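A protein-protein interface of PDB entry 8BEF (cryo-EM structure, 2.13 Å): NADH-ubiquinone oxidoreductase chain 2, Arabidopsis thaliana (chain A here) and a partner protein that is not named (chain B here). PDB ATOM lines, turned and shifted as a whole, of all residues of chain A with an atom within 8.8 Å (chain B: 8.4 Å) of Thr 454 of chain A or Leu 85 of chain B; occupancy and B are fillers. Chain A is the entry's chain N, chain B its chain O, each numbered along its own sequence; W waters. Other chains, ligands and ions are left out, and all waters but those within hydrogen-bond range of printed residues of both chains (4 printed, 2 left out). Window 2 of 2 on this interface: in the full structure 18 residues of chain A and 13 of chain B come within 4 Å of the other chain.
The side-chain carboxylate (OE2) of Glu 94 of chain B lies within salt-bridge range of the side-chain amino group (NZ) of Lys 372 of chain A, 3.1 Å away.
The side-chain carboxylate of Glu 94 of chain B sits at hydrogen-bond distance from the side-chain hydroxyl of Tyr 373 of chain A (3.2 Å).
The guanidinium group of Arg 446 of chain A lies within salt-bridge range of the side-chain carboxylate of Glu 89 of chain B.
NZ of Lys 372 of chain A lies within hydrogen-bond range of OH of Tyr 373 of chain A (3.4 Å).
N of Lys 372 of chain A is in hydrogen-bond range of OD2 of Asp 376 of chain A (3.2 Å).
N of Tyr 373 of chain A lies within hydrogen-bond range of OD2 of Asp 376 of chain A (2.9 Å).
O of Asp 376 of chain A lies within hydrogen-bond range of OH of Tyr 458 of chain A (2.6 Å).
A ring nitrogen (ND1) of His 83 of chain B sits at hydrogen-bond distance from the backbone carbonyl oxygen (O) of Leu 85 of chain B.
The backbone NH (N) of Glu 89 of chain B sits at hydrogen-bond distance from the side-chain carboxylate (OD1) of Asp 87 of chain B (2.9 Å).
Among the printed residues, merely in contact across the chains: Tyr 373 of chain A with Glu 89 of chain B, Tyr 373 of chain A with Ala 90 of chain B, Tyr 373 of chain A with Cys 91 of chain B, Ala 375 of chain A with Leu 85 of chain B, Ala 375 of chain A with Asp 87 of chain B, Asp 376 of chain A with Leu 85 of chain B, Thr 454 of chain A with Arg 84 of chain B and Thr 454 of chain A with Leu 85 of chain B.
Thr 454 of chain A touches two residues of chain B.
Leu 85 of chain B touches just these residues of chain A: Ala 375, Asp 376 and Thr 454.
Of the printed residues of chain B, Arg 446 of chain A touches Glu 89.
Of the printed residues of chain B, Asp 376 of chain A touches Leu 85.
Of the printed residues of chain A, Glu 94 of chain B touches Lys 372 and Tyr 373.
Of the printed residues of chain A, Asp 87 of chain B touches Ala 375.
Of the printed residues of chain B, Ala 375 of chain A touches Leu 85 (3.9 Å) and Asp 87 (3.8 Å).
The nearest residue of chain A that does not touch Leu 85 of chain B is Ile 456 of chain A (4.1 Å).
Hydrophobic or aromatic side chains of chain A within 4 Å of the printed part of chain B: Tyr 373 and Ala 375.
Of the 20 printed residues of chain B, 7 touch a printed residue of chain A.
Hydrophobic or aromatic side chains of chain B that line the printed part of chain A: Leu 85 and Ala 90.
Water W2 lies within hydrogen-bond range of O of Ser 82 of chain B, NZ of Lys 372 of chain A and OE2 of Glu 94 of chain B.
Water W3 bridges the side-chain carboxylate (OD2) of Asp 376 of chain A (2.8 Å) and the guanidinium group (NH2) of Arg 84 of chain B (2.9 Å).
Water W4 bridges NH2 of Arg 84 of chain B and OH of Tyr 458 of chain A.
Water W1 lies within hydrogen-bond range of the backbone carbonyl oxygen of Glu 89 of chain B (2.9 Å), the backbone NH of Ala 375 of chain A (3.1 Å) and the backbone NH of Ile 374 of chain A (3.3 Å).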
ATOM      1  N   LYS A 372      25.323 -18.585  11.850  1.00  0.00           N
ATOM      2  CA  LYS A 372      25.844 -17.871  10.650  1.00  0.00           C
ATOM      3  C   LYS A 372      25.572 -16.382  10.741  1.00  0.00           C
ATOM      4  O   LYS A 372      26.474 -15.649  10.486  1.00  0.00           O
ATOM      5  CB  LYS A 372      25.271 -18.496   9.371  1.00  0.00           C
ATOM      6  CG  LYS A 372      25.677 -17.903   8.041  1.00  0.00           C
ATOM      7  CD  LYS A 372      24.905 -18.573   6.919  1.00  0.00           C
ATOM      8  CE  LYS A 372      25.060 -17.855   5.603  1.00  0.00           C
ATOM      9  NZ  LYS A 372      24.372 -18.530   4.476  1.00  0.00           N
ATOM     10  N   TYR A 373      24.373 -16.019  11.131  1.00  0.00           N
ATOM     11  CA  TYR A 373      24.006 -14.614  11.144  1.00  0.00           C
ATOM     12  C   TYR A 373      23.990 -14.084  12.571  1.00  0.00           C
ATOM     13  O   TYR A 373      23.779 -14.834  13.526  1.00  0.00           O
ATOM     14  CB  TYR A 373      22.628 -14.395  10.511  1.00  0.00           C
ATOM     15  CG  TYR A 373      22.518 -14.821   9.064  1.00  0.00           C
ATOM     16  CD1 TYR A 373      22.909 -13.969   8.037  1.00  0.00           C
ATOM     17  CD2 TYR A 373      22.005 -16.066   8.725  1.00  0.00           C
ATOM     18  CE1 TYR A 373      22.802 -14.352   6.712  1.00  0.00           C
ATOM     19  CE2 TYR A 373      21.896 -16.457   7.406  1.00  0.00           C
ATOM     20  CZ  TYR A 373      22.295 -15.597   6.402  1.00  0.00           C
ATOM     21  OH  TYR A 373      22.184 -15.981   5.087  1.00  0.00           O
ATOM     22  N   ILE A 374      24.205 -12.775  12.701  1.00  0.00           N
ATOM     23  CA  ILE A 374      24.074 -12.128  14.003  1.00  0.00           C
ATOM     24  C   ILE A 374      22.672 -12.339  14.559  1.00  0.00           C
ATOM     25  O   ILE A 374      22.496 -12.605  15.753  1.00  0.00           O
ATOM     26  CB  ILE A 374      24.429 -10.633  13.898  1.00  0.00           C
ATOM     27  CG1 ILE A 374      25.931 -10.455  13.658  1.00  0.00           C
ATOM     28  CG2 ILE A 374      23.995  -9.885  15.148  1.00  0.00           C
ATOM     29  CD1 ILE A 374      26.280  -9.170  12.944  1.00  0.00           C
ATOM     30  N   ALA A 375      21.655 -12.258  13.697  1.00  0.00           N
ATOM     31  CA  ALA A 375      20.278 -12.456  14.135  1.00  0.00           C
ATOM     32  C   ALA A 375      20.029 -13.860  14.680  1.00  0.00           C
ATOM     33  O   ALA A 375      19.072 -14.052  15.437  1.00  0.00           O
ATOM     34  CB  ALA A 375      19.313 -12.163  12.986  1.00  0.00           C
ATOM     35  N   ASP A 376      20.865 -14.839  14.323  1.00  0.00           N
ATOM     36  CA  ASP A 376      20.725 -16.184  14.877  1.00  0.00           C
ATOM     37  C   ASP A 376      20.954 -16.216  16.385  1.00  0.00           C
ATOM     38  O   ASP A 376      20.590 -17.200  17.033  1.00  0.00           O
ATOM     39  CB  ASP A 376      21.697 -17.152  14.195  1.00  0.00           C
ATOM     40  CG  ASP A 376      21.353 -17.411  12.738  1.00  0.00           C
ATOM     41  OD1 ASP A 376      20.175 -17.238  12.355  1.00  0.00           O
ATOM     42  OD2 ASP A 376      22.265 -17.791  11.972  1.00  0.00           O
ATOM     43  N   LEU A 377      21.582 -15.212  16.989  1.00  0.00           N
ATOM     44  CA  LEU A 377      21.810 -15.100  18.442  1.00  0.00           C
ATOM     45  C   LEU A 377      20.536 -14.658  19.203  1.00  0.00           C
ATOM     46  O   LEU A 377      20.650 -14.469  20.379  1.00  0.00           O
ATOM     47  CB  LEU A 377      22.966 -14.113  18.672  1.00  0.00           C
ATOM     48  CG  LEU A 377      24.292 -14.395  17.975  1.00  0.00           C
ATOM     49  CD1 LEU A 377      25.232 -13.210  18.158  1.00  0.00           C
ATOM     50  CD2 LEU A 377      24.908 -15.687  18.470  1.00  0.00           C
ATOM     51  N   GLY A 378      19.423 -14.440  18.522  1.00  0.00           N
ATOM     52  CA  GLY A 378      18.261 -13.915  19.218  1.00  0.00           C
ATOM     53  C   GLY A 378      17.832 -14.821  20.359  1.00  0.00           C
ATOM     54  O   GLY A 378      17.912 -16.048  20.271  1.00  0.00           O
ATOM     55  N   ALA A 379      17.390 -14.197  21.453  1.00  0.00           N
ATOM     56  CA  ALA A 379      16.889 -14.879  22.647  1.00  0.00           C
ATOM     57  C   ALA A 379      17.953 -15.735  23.338  1.00  0.00           C
ATOM     58  O   ALA A 379      17.616 -16.589  24.163  1.00  0.00           O
ATOM     59  CB  ALA A 379      15.655 -15.733  22.324  1.00  0.00           C
ATOM     60  N   THR A 383      17.820 -18.725  26.384  1.00  0.00           N
ATOM     61  CA  THR A 383      18.144 -20.135  26.207  1.00  0.00           C
ATOM     62  C   THR A 383      19.476 -20.532  26.832  1.00  0.00           C
ATOM     63  O   THR A 383      19.686 -21.719  27.095  1.00  0.00           O
ATOM     64  CB  THR A 383      18.135 -20.497  24.717  1.00  0.00           C
ATOM     65  OG1 THR A 383      19.167 -19.780  24.029  1.00  0.00           O
ATOM     66  CG2 THR A 383      16.788 -20.157  24.100  1.00  0.00           C
ATOM     67  N   ARG A 446      20.935  -7.901  20.284  1.00  0.00           N
ATOM     68  CA  ARG A 446      20.314  -9.076  19.680  1.00  0.00           C
ATOM     69  C   ARG A 446      20.109 -10.177  20.711  1.00  0.00           C
ATOM     70  O   ARG A 446      19.073 -10.851  20.714  1.00  0.00           O
ATOM     71  CB  ARG A 446      21.166  -9.590  18.519  1.00  0.00           C
ATOM     72  CG  ARG A 446      20.582 -10.801  17.814  1.00  0.00           C
ATOM     73  CD  ARG A 446      19.242 -10.468  17.182  1.00  0.00           C
ATOM     74  NE  ARG A 446      19.401  -9.585  16.034  1.00  0.00           N
ATOM     75  CZ  ARG A 446      18.469  -9.368  15.117  1.00  0.00           C
ATOM     76  NH1 ARG A 446      17.278  -9.942  15.192  1.00  0.00           N
ATOM     77  NH2 ARG A 446      18.740  -8.562  14.097  1.00  0.00           N
ATOM     78  N   THR A 451      12.947  -9.870  20.727  1.00  0.00           N
ATOM     79  CA  THR A 451      11.951 -10.915  20.967  1.00  0.00           C
ATOM     80  C   THR A 451      11.545 -11.508  19.624  1.00  0.00           C
ATOM     81  O   THR A 451      10.488 -11.173  19.075  1.00  0.00           O
ATOM     82  CB  THR A 451      10.740 -10.366  21.726  1.00  0.00           C
ATOM     83  OG1 THR A 451      10.263  -9.181  21.078  1.00  0.00           O
ATOM     84  CG2 THR A 451      11.120 -10.028  23.157  1.00  0.00           C
ATOM     85  N   PRO A 452      12.366 -12.391  19.061  1.00  0.00           N
ATOM     86  CA  PRO A 452      12.044 -12.968  17.751  1.00  0.00           C
ATOM     87  C   PRO A 452      10.928 -13.997  17.844  1.00  0.00           C
ATOM     88  O   PRO A 452      10.658 -14.578  18.895  1.00  0.00           O
ATOM     89  CB  PRO A 452      13.356 -13.622  17.305  1.00  0.00           C
ATOM     90  CG  PRO A 452      14.266 -13.606  18.491  1.00  0.00           C
ATOM     91  CD  PRO A 452      13.572 -12.984  19.658  1.00  0.00           C
ATOM     92  N   ARG A 453      10.275 -14.217  16.702  1.00  0.00           N
ATOM     93  CA  ARG A 453       9.197 -15.198  16.644  1.00  0.00           C
ATOM     94  C   ARG A 453       9.743 -16.622  16.661  1.00  0.00           C
ATOM     95  O   ARG A 453       9.179 -17.502  17.319  1.00  0.00           O
ATOM     96  CB  ARG A 453       8.339 -14.954  15.402  1.00  0.00           C
ATOM     97  CG  ARG A 453       7.359 -16.068  15.072  1.00  0.00           C
ATOM     98  CD  ARG A 453       6.391 -16.330  16.219  1.00  0.00           C
ATOM     99  NE  ARG A 453       5.489 -17.439  15.927  1.00  0.00           N
ATOM    100  CZ  ARG A 453       5.758 -18.713  16.177  1.00  0.00           C
ATOM    101  NH1 ARG A 453       6.906 -19.082  16.719  1.00  0.00           N
ATOM    102  NH2 ARG A 453       4.854 -19.640  15.869  1.00  0.00           N
ATOM    103  N   THR A 454      10.839 -16.867  15.949  1.00  0.00           N
ATOM    104  CA  THR A 454      11.483 -18.173  15.914  1.00  0.00           C
ATOM    105  C   THR A 454      12.824 -18.092  16.632  1.00  0.00           C
ATOM    106  O   THR A 454      13.634 -17.205  16.346  1.00  0.00           O
ATOM    107  CB  THR A 454      11.676 -18.656  14.472  1.00  0.00           C
ATOM    108  OG1 THR A 454      10.402 -18.956  13.892  1.00  0.00           O
ATOM    109  CG2 THR A 454      12.543 -19.908  14.430  1.00  0.00           C
ATOM    110  N   TRP A 455      13.045 -19.007  17.568  1.00  0.00           N
ATOM    111  CA  TRP A 455      14.296 -19.099  18.305  1.00  0.00           C
ATOM    112  C   TRP A 455      15.142 -20.240  17.755  1.00  0.00           C
ATOM    113  O   TRP A 455      14.623 -21.211  17.202  1.00  0.00           O
ATOM    114  CB  TRP A 455      14.047 -19.335  19.798  1.00  0.00           C
ATOM    115  CG  TRP A 455      13.305 -18.245  20.515  1.00  0.00           C
ATOM    116  CD1 TRP A 455      12.680 -17.168  19.963  1.00  0.00           C
ATOM    117  CD2 TRP A 455      13.102 -18.143  21.929  1.00  0.00           C
ATOM    118  NE1 TRP A 455      12.105 -16.399  20.944  1.00  0.00           N
ATOM    119  CE2 TRP A 455      12.350 -16.977  22.161  1.00  0.00           C
ATOM    120  CE3 TRP A 455      13.489 -18.925  23.022  1.00  0.00           C
ATOM    121  CZ2 TRP A 455      11.980 -16.572  23.440  1.00  0.00           C
ATOM    122  CZ3 TRP A 455      13.119 -18.521  24.291  1.00  0.00           C
ATOM    123  CH2 TRP A 455      12.371 -17.355  24.489  1.00  0.00           C
ATOM    124  N   ILE A 456      16.455 -20.114  17.912  1.00  0.00           N
ATOM    125  CA  ILE A 456      17.383 -21.203  17.639  1.00  0.00           C
ATOM    126  C   ILE A 456      17.936 -21.675  18.976  1.00  0.00           C
ATOM    127  O   ILE A 456      18.516 -20.886  19.731  1.00  0.00           O
ATOM    128  CB  ILE A 456      18.512 -20.777  16.691  1.00  0.00           C
ATOM    129  CG1 ILE A 456      17.984 -20.653  15.261  1.00  0.00           C
ATOM    130  CG2 ILE A 456      19.650 -21.789  16.735  1.00  0.00           C
ATOM    131  CD1 ILE A 456      18.755 -19.673  14.417  1.00  0.00           C
ATOM    132  N   LEU A 457      17.751 -22.957  19.272  1.00  0.00           N
ATOM    133  CA  LEU A 457      18.257 -23.552  20.501  1.00  0.00           C
ATOM    134  C   LEU A 457      19.612 -24.188  20.213  1.00  0.00           C
ATOM    135  O   LEU A 457      19.725 -25.034  19.323  1.00  0.00           O
ATOM    136  CB  LEU A 457      17.269 -24.584  21.045  1.00  0.00           C
ATOM    137  CG  LEU A 457      15.810 -24.116  21.106  1.00  0.00           C
ATOM    138  CD1 LEU A 457      14.904 -25.176  21.723  1.00  0.00           C
ATOM    139  CD2 LEU A 457      15.701 -22.805  21.863  1.00  0.00           C
ATOM    140  N   TYR A 458      20.631 -23.791  20.968  1.00  0.00           N
ATOM    141  CA  TYR A 458      22.000 -24.213  20.711  1.00  0.00           C
ATOM    142  C   TYR A 458      22.401 -25.365  21.626  1.00  0.00           C
ATOM    143  O   TYR A 458      22.010 -25.413  22.794  1.00  0.00           O
ATOM    144  CB  TYR A 458      22.966 -23.039  20.882  1.00  0.00           C
ATOM    145  CG  TYR A 458      22.807 -21.989  19.810  1.00  0.00           C
ATOM    146  CD1 TYR A 458      23.494 -22.090  18.609  1.00  0.00           C
ATOM    147  CD2 TYR A 458      21.954 -20.909  19.989  1.00  0.00           C
ATOM    148  CE1 TYR A 458      23.346 -21.143  17.621  1.00  0.00           C
ATOM    149  CE2 TYR A 458      21.798 -19.954  19.008  1.00  0.00           C
ATOM    150  CZ  TYR A 458      22.498 -20.074  17.824  1.00  0.00           C
ATOM    151  OH  TYR A 458      22.345 -19.127  16.842  1.00  0.00           O
ATOM    152  N   THR B  67       4.952 -17.265   5.676  1.00  0.00           N
ATOM    153  CA  THR B  67       5.709 -16.862   4.501  1.00  0.00           C
ATOM    154  C   THR B  67       5.700 -17.948   3.425  1.00  0.00           C
ATOM    155  O   THR B  67       5.476 -19.131   3.693  1.00  0.00           O
ATOM    156  CB  THR B  67       7.153 -16.512   4.874  1.00  0.00           C
ATOM    157  OG1 THR B  67       7.839 -17.684   5.333  1.00  0.00           O
ATOM    158  CG2 THR B  67       7.188 -15.437   5.959  1.00  0.00           C
ATOM    159  N   LEU B  69       8.291 -18.963   1.997  1.00  0.00           N
ATOM    160  CA  LEU B  69       9.413 -19.839   2.315  1.00  0.00           C
ATOM    161  C   LEU B  69       8.970 -21.021   3.170  1.00  0.00           C
ATOM    162  O   LEU B  69       9.414 -22.149   2.948  1.00  0.00           O
ATOM    163  CB  LEU B  69      10.513 -19.048   3.024  1.00  0.00           C
ATOM    164  CG  LEU B  69      11.597 -19.891   3.704  1.00  0.00           C
ATOM    165  CD1 LEU B  69      12.399 -20.677   2.671  1.00  0.00           C
ATOM    166  CD2 LEU B  69      12.504 -19.027   4.566  1.00  0.00           C
ATOM    167  N   ARG B  70       8.108 -20.782   4.160  1.00  0.00           N
ATOM    168  CA  ARG B  70       7.632 -21.873   5.007  1.00  0.00           C
ATOM    169  C   ARG B  70       6.853 -22.904   4.197  1.00  0.00           C
ATOM    170  O   ARG B  70       7.053 -24.121   4.350  1.00  0.00           O
ATOM    171  CB  ARG B  70       6.766 -21.315   6.135  1.00  0.00           C
ATOM    172  CG  ARG B  70       6.166 -22.377   7.029  1.00  0.00           C
ATOM    173  CD  ARG B  70       7.225 -22.950   7.950  1.00  0.00           C
ATOM    174  NE  ARG B  70       8.036 -21.895   8.543  1.00  0.00           N
ATOM    175  CZ  ARG B  70       7.635 -21.101   9.527  1.00  0.00           C
ATOM    176  NH1 ARG B  70       6.428 -21.212  10.057  1.00  0.00           N
ATOM    177  NH2 ARG B  70       8.464 -20.169   9.986  1.00  0.00           N
ATOM    178  N   PRO B  80      14.901 -26.423   4.687  1.00  0.00           N
ATOM    179  CA  PRO B  80      14.635 -25.578   5.864  1.00  0.00           C
ATOM    180  C   PRO B  80      15.891 -25.196   6.625  1.00  0.00           C
ATOM    181  O   PRO B  80      15.962 -24.087   7.166  1.00  0.00           O
ATOM    182  CB  PRO B  80      13.692 -26.443   6.716  1.00  0.00           C
ATOM    183  CG  PRO B  80      13.869 -27.835   6.217  1.00  0.00           C
ATOM    184  CD  PRO B  80      14.234 -27.733   4.774  1.00  0.00           C
ATOM    185  N   ALA B  81      16.891 -26.081   6.670  1.00  0.00           N
ATOM    186  CA  ALA B  81      18.135 -25.780   7.369  1.00  0.00           C
ATOM    187  C   ALA B  81      18.879 -24.602   6.754  1.00  0.00           C
ATOM    188  O   ALA B  81      19.672 -23.958   7.444  1.00  0.00           O
ATOM    189  CB  ALA B  81      19.039 -27.015   7.381  1.00  0.00           C
ATOM    190  N   SER B  82      18.645 -24.308   5.475  1.00  0.00           N
ATOM    191  CA  SER B  82      19.346 -23.216   4.815  1.00  0.00           C
ATOM    192  C   SER B  82      18.750 -21.850   5.129  1.00  0.00           C
ATOM    193  O   SER B  82      19.403 -20.834   4.877  1.00  0.00           O
ATOM    194  CB  SER B  82      19.352 -23.436   3.302  1.00  0.00           C
ATOM    195  OG  SER B  82      18.132 -23.013   2.721  1.00  0.00           O
ATOM    196  N   HIS B  83      17.530 -21.800   5.654  1.00  0.00           N
ATOM    197  CA  HIS B  83      16.877 -20.525   5.956  1.00  0.00           C
ATOM    198  C   HIS B  83      15.943 -20.777   7.141  1.00  0.00           C
ATOM    199  O   HIS B  83      14.766 -21.092   6.957  1.00  0.00           O
ATOM    200  CB  HIS B  83      16.126 -20.023   4.732  1.00  0.00           C
ATOM    201  CG  HIS B  83      15.901 -18.547   4.705  1.00  0.00           C
ATOM    202  ND1 HIS B  83      15.481 -17.828   5.804  1.00  0.00           N
ATOM    203  CD2 HIS B  83      16.031 -17.653   3.700  1.00  0.00           C
ATOM    204  CE1 HIS B  83      15.364 -16.555   5.473  1.00  0.00           C
ATOM    205  NE2 HIS B  83      15.695 -16.421   4.203  1.00  0.00           N
ATOM    206  N   ARG B  84      16.470 -20.597   8.348  1.00  0.00           N
ATOM    207  CA  ARG B  84      15.750 -21.017   9.544  1.00  0.00           C
ATOM    208  C   ARG B  84      14.886 -19.920  10.148  1.00  0.00           C
ATOM    209  O   ARG B  84      13.934 -20.232  10.870  1.00  0.00           O
ATOM    210  CB  ARG B  84      16.734 -21.539  10.594  1.00  0.00           C
ATOM    211  CG  ARG B  84      17.123 -22.998  10.375  1.00  0.00           C
ATOM    212  CD  ARG B  84      18.129 -23.492  11.396  1.00  0.00           C
ATOM    213  NE  ARG B  84      19.394 -22.775  11.321  1.00  0.00           N
ATOM    214  CZ  ARG B  84      20.385 -22.915  12.190  1.00  0.00           C
ATOM    215  NH1 ARG B  84      20.299 -23.758  13.205  1.00  0.00           N
ATOM    216  NH2 ARG B  84      21.492 -22.198  12.031  1.00  0.00           N
ATOM    217  N   LEU B  85      15.192 -18.657   9.877  1.00  0.00           N
ATOM    218  CA  LEU B  85      14.375 -17.537  10.319  1.00  0.00           C
ATOM    219  C   LEU B  85      13.694 -16.894   9.118  1.00  0.00           C
ATOM    220  O   LEU B  85      14.137 -17.039   7.981  1.00  0.00           O
ATOM    221  CB  LEU B  85      15.219 -16.499  11.065  1.00  0.00           C
ATOM    222  CG  LEU B  85      16.177 -17.039  12.130  1.00  0.00           C
ATOM    223  CD1 LEU B  85      17.054 -15.927  12.678  1.00  0.00           C
ATOM    224  CD2 LEU B  85      15.403 -17.718  13.246  1.00  0.00           C
ATOM    225  N   ASP B  86      12.599 -16.183   9.382  1.00  0.00           N
ATOM    226  CA  ASP B  86      11.886 -15.433   8.354  1.00  0.00           C
ATOM    227  C   ASP B  86      12.259 -13.955   8.362  1.00  0.00           C
ATOM    228  O   ASP B  86      11.409 -13.098   8.096  1.00  0.00           O
ATOM    229  CB  ASP B  86      10.376 -15.596   8.520  1.00  0.00           C
ATOM    230  CG  ASP B  86       9.887 -16.974   8.122  1.00  0.00           C
ATOM    231  OD1 ASP B  86      10.152 -17.397   6.977  1.00  0.00           O
ATOM    232  OD2 ASP B  86       9.231 -17.632   8.952  1.00  0.00           O
ATOM    233  N   ASP B  87      13.517 -13.644   8.658  1.00  0.00           N
ATOM    234  CA  ASP B  87      13.986 -12.280   8.846  1.00  0.00           C
ATOM    235  C   ASP B  87      14.944 -11.903   7.724  1.00  0.00           C
ATOM    236  O   ASP B  87      15.776 -12.715   7.303  1.00  0.00           O
ATOM    237  CB  ASP B  87      14.674 -12.134  10.211  1.00  0.00           C
ATOM    238  CG  ASP B  87      15.368 -10.792  10.392  1.00  0.00           C
ATOM    239  OD1 ASP B  87      15.055  -9.822   9.670  1.00  0.00           O
ATOM    240  OD2 ASP B  87      16.241 -10.708  11.278  1.00  0.00           O
ATOM    241  N   ILE B  88      14.824 -10.662   7.248  1.00  0.00           N
ATOM    242  CA  ILE B  88      15.679 -10.183   6.167  1.00  0.00           C
ATOM    243  C   ILE B  88      17.137 -10.101   6.616  1.00  0.00           C
ATOM    244  O   ILE B  88      18.053 -10.204   5.792  1.00  0.00           O
ATOM    245  CB  ILE B  88      15.157  -8.827   5.647  1.00  0.00           C
ATOM    246  CG1 ILE B  88      15.932  -8.386   4.406  1.00  0.00           C
ATOM    247  CG2 ILE B  88      15.217  -7.769   6.728  1.00  0.00           C
ATOM    248  CD1 ILE B  88      15.847  -9.360   3.273  1.00  0.00           C
ATOM    249  N   GLU B  89      17.380  -9.932   7.917  1.00  0.00           N
ATOM    250  CA  GLU B  89      18.742  -9.867   8.434  1.00  0.00           C
ATOM    251  C   GLU B  89      19.429 -11.227   8.471  1.00  0.00           C
ATOM    252  O   GLU B  89      20.640 -11.282   8.703  1.00  0.00           O
ATOM    253  CB  GLU B  89      18.741  -9.251   9.834  1.00  0.00           C
ATOM    254  CG  GLU B  89      18.101  -7.881   9.906  1.00  0.00           C
ATOM    255  CD  GLU B  89      18.204  -7.266  11.285  1.00  0.00           C
ATOM    256  OE1 GLU B  89      19.335  -6.958  11.717  1.00  0.00           O
ATOM    257  OE2 GLU B  89      17.156  -7.092  11.939  1.00  0.00           O
ATOM    258  N   ALA B  90      18.699 -12.313   8.255  1.00  0.00           N
ATOM    259  CA  ALA B  90      19.269 -13.652   8.196  1.00  0.00           C
ATOM    260  C   ALA B  90      19.024 -14.273   6.827  1.00  0.00           C
ATOM    261  O   ALA B  90      18.655 -15.443   6.709  1.00  0.00           O
ATOM    262  CB  ALA B  90      18.704 -14.535   9.305  1.00  0.00           C
ATOM    263  N   CYS B  91      19.229 -13.491   5.771  1.00  0.00           N
ATOM    264  CA  CYS B  91      18.873 -13.900   4.419  1.00  0.00           C
ATOM    265  C   CYS B  91      20.023 -13.624   3.463  1.00  0.00           C
ATOM    266  O   CYS B  91      20.526 -12.500   3.396  1.00  0.00           O
ATOM    267  CB  CYS B  91      17.611 -13.170   3.941  1.00  0.00           C
ATOM    268  SG  CYS B  91      17.195 -13.468   2.208  1.00  0.00           S
ATOM    269  N   GLU B  94      18.679 -17.398  -0.131  1.00  0.00           N
ATOM    270  CA  GLU B  94      18.368 -18.821  -0.201  1.00  0.00           C
ATOM    271  C   GLU B  94      16.884 -19.062  -0.445  1.00  0.00           C
ATOM    272  O   GLU B  94      16.514 -20.112  -0.979  1.00  0.00           O
ATOM    273  CB  GLU B  94      18.811 -19.527   1.083  1.00  0.00           C
ATOM    274  CG  GLU B  94      20.300 -19.426   1.378  1.00  0.00           C
ATOM    275  CD  GLU B  94      20.645 -18.225   2.237  1.00  0.00           C
ATOM    276  OE1 GLU B  94      19.767 -17.361   2.445  1.00  0.00           O
ATOM    277  OE2 GLU B  94      21.794 -18.146   2.709  1.00  0.00           O
ATOM    278  N   CYS B  95      16.033 -18.108  -0.076  1.00  0.00           N
ATOM    279  CA  CYS B  95      14.592 -18.195  -0.261  1.00  0.00           C
ATOM    280  C   CYS B  95      14.127 -17.658  -1.608  1.00  0.00           C
ATOM    281  O   CYS B  95      12.918 -17.623  -1.853  1.00  0.00           O
ATOM    282  CB  CYS B  95      13.879 -17.416   0.843  1.00  0.00           C
ATOM    283  SG  CYS B  95      14.393 -15.692   0.900  1.00  0.00           S
ATOM    284  N   GLY B 134      11.551 -15.216  -0.869  1.00  0.00           N
ATOM    285  CA  GLY B 134      10.442 -15.992  -0.340  1.00  0.00           C
ATOM    286  C   GLY B 134      10.147 -15.713   1.119  1.00  0.00           C
ATOM    287  O   GLY B 134       9.003 -15.845   1.560  1.00  0.00           O
ATOM    288  N   CYS B 135      11.165 -15.320   1.888  1.00  0.00           N
ATOM    289  CA  CYS B 135      10.960 -15.019   3.298  1.00  0.00           C
ATOM    290  C   CYS B 135      10.218 -13.707   3.514  1.00  0.00           C
ATOM    291  O   CYS B 135       9.735 -13.464   4.623  1.00  0.00           O
ATOM    292  CB  CYS B 135      12.304 -14.980   4.033  1.00  0.00           C
ATOM    293  SG  CYS B 135      13.331 -13.531   3.673  1.00  0.00           S
ATOM    294  N   GLN B 136      10.122 -12.857   2.493  1.00  0.00           N
ATOM    295  CA  GLN B 136       9.430 -11.580   2.609  1.00  0.00           C
ATOM    296  C   GLN B 136       8.045 -11.584   1.973  1.00  0.00           C
ATOM    297  O   GLN B 136       7.388 -10.540   1.956  1.00  0.00           O
ATOM    298  CB  GLN B 136      10.275 -10.461   1.988  1.00  0.00           C
ATOM    299  CG  GLN B 136      11.658 -10.332   2.590  1.00  0.00           C
ATOM    300  CD  GLN B 136      11.615  -9.902   4.040  1.00  0.00           C
ATOM    301  OE1 GLN B 136      11.267  -8.765   4.350  1.00  0.00           O
ATOM    302  NE2 GLN B 136      11.966 -10.814   4.938  1.00  0.00           N
HETATM  303  O   HOH W   1      22.195 -10.669  11.050  1.00  0.00           O
HETATM  304  O   HOH W   2      21.859 -19.622   5.458  1.00  0.00           O
HETATM  305  O   HOH W   3      21.692 -19.936  10.260  1.00  0.00           O
HETATM  306  O   HOH W   4      22.265 -20.763  14.381  1.00  0.00           O
